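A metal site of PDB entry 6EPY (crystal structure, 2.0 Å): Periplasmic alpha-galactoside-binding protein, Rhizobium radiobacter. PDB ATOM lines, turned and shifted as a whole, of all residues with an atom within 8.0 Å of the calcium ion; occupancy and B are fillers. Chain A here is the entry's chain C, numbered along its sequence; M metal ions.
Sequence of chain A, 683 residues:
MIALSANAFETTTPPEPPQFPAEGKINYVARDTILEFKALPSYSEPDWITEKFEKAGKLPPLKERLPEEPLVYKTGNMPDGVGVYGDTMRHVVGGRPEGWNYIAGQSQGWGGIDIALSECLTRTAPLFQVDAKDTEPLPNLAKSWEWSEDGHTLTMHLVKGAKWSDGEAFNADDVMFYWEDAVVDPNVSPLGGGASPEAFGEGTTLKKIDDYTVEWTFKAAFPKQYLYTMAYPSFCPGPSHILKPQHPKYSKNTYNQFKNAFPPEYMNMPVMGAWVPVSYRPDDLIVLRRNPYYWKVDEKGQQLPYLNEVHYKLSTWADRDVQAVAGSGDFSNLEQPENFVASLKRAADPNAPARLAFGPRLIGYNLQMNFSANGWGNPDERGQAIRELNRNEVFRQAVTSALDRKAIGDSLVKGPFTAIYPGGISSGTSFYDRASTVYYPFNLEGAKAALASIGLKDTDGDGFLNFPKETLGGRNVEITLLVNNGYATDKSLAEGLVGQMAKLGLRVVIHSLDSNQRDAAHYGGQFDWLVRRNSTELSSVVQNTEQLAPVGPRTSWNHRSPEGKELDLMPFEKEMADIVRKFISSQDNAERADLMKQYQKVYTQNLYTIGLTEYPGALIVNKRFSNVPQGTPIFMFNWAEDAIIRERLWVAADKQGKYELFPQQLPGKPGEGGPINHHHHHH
The calcium ion is bound by OD1 of Asn 466 (2.1 Å), OD1 of Asn 476 (2.3 Å), O of Phe 464 (2.4 Å), OD1 of Asp 458 (2.7 Å) and OD1 of Asp 462 (2.7 Å).
The calcium ion has five donor atoms within binding distance.
The side-chain carboxylate of Asp 460 is in hydrogen-bond range of the side-chain amide nitrogen of Asn 466 (2.9 Å).
The side-chain amide oxygen (OD1) of Asn 466 sits close to the backbone NH (N) of Thr 459.
The backbone NH (N) of Asn 466 sits at hydrogen-bond distance from the backbone carbonyl oxygen (O) of Lys 457 (2.9 Å).
The side-chain amide nitrogen (ND2) of Asn 466 is in hydrogen-bond range of the backbone carbonyl oxygen (O) of Gly 474 (3.0 Å).
The side-chain carboxylate of Asp 458 lies close to the backbone NH of Gly 461 (3.1 Å).
The side-chain carboxylate (OD2) of Asp 458 lies within hydrogen-bond range of the backbone NH (N) of Gly 463 (2.8 Å).
OG1 of Thr 459 is in hydrogen-bond range of OD1 of Asp 460 (3.3 Å).
Residues that only touch the calcium ion: Asp 460 (3.4 Å).
Of the 16 residues printed, 6 come within 4 Å of the calcium ion.
Along chain A the residues within 4 Å of the calcium ion span positions 458 to 476.
The nearest printed residue that does not touch the calcium ion is Thr 459 (4.3 Å).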
ATOM      1  N   LYS A 457      27.439   7.040  10.480  1.00  0.00           N
ATOM      2  CA  LYS A 457      27.479   5.940  11.455  1.00  0.00           C
ATOM      3  C   LYS A 457      26.668   4.739  11.009  1.00  0.00           C
ATOM      4  O   LYS A 457      25.670   4.894  10.302  1.00  0.00           O
ATOM      5  CB  LYS A 457      27.100   6.402  12.888  1.00  0.00           C
ATOM      6  CG  LYS A 457      25.643   6.859  13.095  1.00  0.00           C
ATOM      7  CD  LYS A 457      25.324   7.086  14.570  1.00  0.00           C
ATOM      8  CE  LYS A 457      25.150   8.549  14.902  1.00  0.00           C
ATOM      9  NZ  LYS A 457      25.201   8.786  16.366  1.00  0.00           N
ATOM     10  N   ASP A 458      27.116   3.541  11.385  1.00  0.00           N
ATOM     11  CA  ASP A 458      26.426   2.287  11.048  1.00  0.00           C
ATOM     12  C   ASP A 458      25.286   2.060  12.042  1.00  0.00           C
ATOM     13  O   ASP A 458      25.514   1.603  13.174  1.00  0.00           O
ATOM     14  CB  ASP A 458      27.409   1.109  11.013  1.00  0.00           C
ATOM     15  CG  ASP A 458      26.816  -0.253  10.709  1.00  0.00           C
ATOM     16  OD1 ASP A 458      25.713  -0.308  10.108  1.00  0.00           O
ATOM     17  OD2 ASP A 458      27.468  -1.263  11.026  1.00  0.00           O
ATOM     18  N   THR A 459      24.062   2.381  11.623  1.00  0.00           N
ATOM     19  CA  THR A 459      22.855   2.256  12.443  1.00  0.00           C
ATOM     20  C   THR A 459      22.307   0.819  12.510  1.00  0.00           C
ATOM     21  O   THR A 459      21.747   0.425  13.557  1.00  0.00           O
ATOM     22  CB  THR A 459      21.774   3.259  11.977  1.00  0.00           C
ATOM     23  OG1 THR A 459      21.314   2.891  10.682  1.00  0.00           O
ATOM     24  CG2 THR A 459      22.266   4.703  11.959  1.00  0.00           C
ATOM     25  N   ASP A 460      22.441   0.054  11.400  1.00  0.00           N
ATOM     26  CA  ASP A 460      21.911  -1.314  11.193  1.00  0.00           C
ATOM     27  C   ASP A 460      22.860  -2.463  11.566  1.00  0.00           C
ATOM     28  O   ASP A 460      22.457  -3.628  11.510  1.00  0.00           O
ATOM     29  CB  ASP A 460      21.436  -1.493   9.734  1.00  0.00           C
ATOM     30  CG  ASP A 460      20.766  -0.277   9.123  1.00  0.00           C
ATOM     31  OD1 ASP A 460      19.709   0.147   9.648  1.00  0.00           O
ATOM     32  OD2 ASP A 460      21.301   0.242   8.114  1.00  0.00           O
ATOM     33  N   GLY A 461      24.098  -2.153  11.925  1.00  0.00           N
ATOM     34  CA  GLY A 461      25.095  -3.149  12.307  1.00  0.00           C
ATOM     35  C   GLY A 461      25.570  -4.076  11.201  1.00  0.00           C
ATOM     36  O   GLY A 461      25.967  -5.205  11.497  1.00  0.00           O
ATOM     37  N   ASP A 462      25.542  -3.615   9.926  1.00  0.00           N
ATOM     38  CA  ASP A 462      26.024  -4.381   8.761  1.00  0.00           C
ATOM     39  C   ASP A 462      27.493  -4.081   8.395  1.00  0.00           C
ATOM     40  O   ASP A 462      27.993  -4.545   7.368  1.00  0.00           O
ATOM     41  CB  ASP A 462      25.079  -4.223   7.548  1.00  0.00           C
ATOM     42  CG  ASP A 462      25.072  -2.882   6.827  1.00  0.00           C
ATOM     43  OD1 ASP A 462      25.678  -1.910   7.342  1.00  0.00           O
ATOM     44  OD2 ASP A 462      24.430  -2.784   5.756  1.00  0.00           O
ATOM     45  N   GLY A 463      28.173  -3.300   9.234  1.00  0.00           N
ATOM     46  CA  GLY A 463      29.568  -2.929   9.042  1.00  0.00           C
ATOM     47  C   GLY A 463      29.781  -1.731   8.133  1.00  0.00           C
ATOM     48  O   GLY A 463      30.911  -1.249   8.019  1.00  0.00           O
ATOM     49  N   PHE A 464      28.707  -1.255   7.463  1.00  0.00           N
ATOM     50  CA  PHE A 464      28.770  -0.109   6.554  1.00  0.00           C
ATOM     51  C   PHE A 464      28.115   1.122   7.137  1.00  0.00           C
ATOM     52  O   PHE A 464      27.066   1.019   7.760  1.00  0.00           O
ATOM     53  CB  PHE A 464      28.188  -0.452   5.172  1.00  0.00           C
ATOM     54  CG  PHE A 464      29.031  -1.430   4.404  1.00  0.00           C
ATOM     55  CD1 PHE A 464      30.243  -1.026   3.821  1.00  0.00           C
ATOM     56  CD2 PHE A 464      28.650  -2.760   4.267  1.00  0.00           C
ATOM     57  CE1 PHE A 464      31.038  -1.943   3.126  1.00  0.00           C
ATOM     58  CE2 PHE A 464      29.436  -3.669   3.565  1.00  0.00           C
ATOM     59  CZ  PHE A 464      30.633  -3.256   2.996  1.00  0.00           C
ATOM     60  N   LEU A 465      28.711   2.296   6.927  1.00  0.00           N
ATOM     61  CA  LEU A 465      28.192   3.551   7.441  1.00  0.00           C
ATOM     62  C   LEU A 465      26.985   4.063   6.668  1.00  0.00           C
ATOM     63  O   LEU A 465      26.951   3.978   5.446  1.00  0.00           O
ATOM     64  CB  LEU A 465      29.289   4.626   7.500  1.00  0.00           C
ATOM     65  CG  LEU A 465      30.592   4.266   8.235  1.00  0.00           C
ATOM     66  CD1 LEU A 465      31.687   5.219   7.851  1.00  0.00           C
ATOM     67  CD2 LEU A 465      30.410   4.266   9.735  1.00  0.00           C
ATOM     68  N   ASN A 466      25.994   4.596   7.407  1.00  0.00           N
ATOM     69  CA  ASN A 466      24.773   5.182   6.875  1.00  0.00           C
ATOM     70  C   ASN A 466      24.875   6.713   6.909  1.00  0.00           C
ATOM     71  O   ASN A 466      25.506   7.276   7.805  1.00  0.00           O
ATOM     72  CB  ASN A 466      23.547   4.771   7.720  1.00  0.00           C
ATOM     73  CG  ASN A 466      23.275   3.294   7.749  1.00  0.00           C
ATOM     74  OD1 ASN A 466      24.062   2.498   8.261  1.00  0.00           O
ATOM     75  ND2 ASN A 466      22.126   2.904   7.203  1.00  0.00           N
ATOM     76  N   PHE A 467      24.188   7.371   5.962  1.00  0.00           N
ATOM     77  CA  PHE A 467      24.068   8.825   5.900  1.00  0.00           C
ATOM     78  C   PHE A 467      23.170   9.268   7.084  1.00  0.00           C
ATOM     79  O   PHE A 467      22.335   8.463   7.517  1.00  0.00           O
ATOM     80  CB  PHE A 467      23.332   9.225   4.601  1.00  0.00           C
ATOM     81  CG  PHE A 467      24.175   9.298   3.362  1.00  0.00           C
ATOM     82  CD1 PHE A 467      25.046  10.361   3.157  1.00  0.00           C
ATOM     83  CD2 PHE A 467      24.043   8.345   2.359  1.00  0.00           C
ATOM     84  CE1 PHE A 467      25.814  10.439   1.988  1.00  0.00           C
ATOM     85  CE2 PHE A 467      24.808   8.440   1.185  1.00  0.00           C
ATOM     86  CZ  PHE A 467      25.676   9.483   1.016  1.00  0.00           C
ATOM     87  N   GLY A 474      18.481   8.118   5.463  1.00  0.00           N
ATOM     88  CA  GLY A 474      19.401   7.344   6.282  1.00  0.00           C
ATOM     89  C   GLY A 474      19.904   6.064   5.647  1.00  0.00           C
ATOM     90  O   GLY A 474      20.257   5.125   6.357  1.00  0.00           O
ATOM     91  N   ARG A 475      19.951   6.020   4.303  1.00  0.00           N
ATOM     92  CA  ARG A 475      20.462   4.876   3.539  1.00  0.00           C
ATOM     93  C   ARG A 475      21.968   4.712   3.767  1.00  0.00           C
ATOM     94  O   ARG A 475      22.645   5.685   4.140  1.00  0.00           O
ATOM     95  CB  ARG A 475      20.242   5.113   2.029  1.00  0.00           C
ATOM     96  CG  ARG A 475      18.859   4.717   1.514  1.00  0.00           C
ATOM     97  CD  ARG A 475      18.767   5.016   0.031  1.00  0.00           C
ATOM     98  NE  ARG A 475      17.507   5.683  -0.317  1.00  0.00           N
ATOM     99  CZ  ARG A 475      17.247   6.241  -1.500  1.00  0.00           C
ATOM    100  NH1 ARG A 475      18.161   6.224  -2.459  1.00  0.00           N
ATOM    101  NH2 ARG A 475      16.078   6.823  -1.724  1.00  0.00           N
ATOM    102  N   ASN A 476      22.499   3.508   3.507  1.00  0.00           N
ATOM    103  CA  ASN A 476      23.940   3.246   3.587  1.00  0.00           C
ATOM    104  C   ASN A 476      24.658   4.098   2.521  1.00  0.00           C
ATOM    105  O   ASN A 476      24.104   4.311   1.433  1.00  0.00           O
ATOM    106  CB  ASN A 476      24.242   1.762   3.310  1.00  0.00           C
ATOM    107  CG  ASN A 476      24.180   0.836   4.502  1.00  0.00           C
ATOM    108  OD1 ASN A 476      24.275   1.245   5.665  1.00  0.00           O
ATOM    109  ND2 ASN A 476      24.071  -0.448   4.237  1.00  0.00           N
ATOM    110  N   VAL A 477      25.869   4.616   2.848  1.00  0.00           N
ATOM    111  CA  VAL A 477      26.682   5.403   1.921  1.00  0.00           C
ATOM    112  C   VAL A 477      27.112   4.446   0.821  1.00  0.00           C
ATOM    113  O   VAL A 477      27.596   3.354   1.109  1.00  0.00           O
ATOM    114  CB  VAL A 477      27.889   6.118   2.608  1.00  0.00           C
ATOM    115  CG1 VAL A 477      28.753   6.871   1.593  1.00  0.00           C
ATOM    116  CG2 VAL A 477      27.403   7.067   3.710  1.00  0.00           C
ATOM    117  N   GLY A 505      34.576   1.355   6.560  1.00  0.00           N
ATOM    118  CA  GLY A 505      33.122   1.352   6.687  1.00  0.00           C
ATOM    119  C   GLY A 505      32.380   1.915   5.488  1.00  0.00           C
ATOM    120  O   GLY A 505      31.156   2.067   5.553  1.00  0.00           O
HETATM  121 CA    CA M   1      24.688   0.519   7.800  1.00  0.00          CA
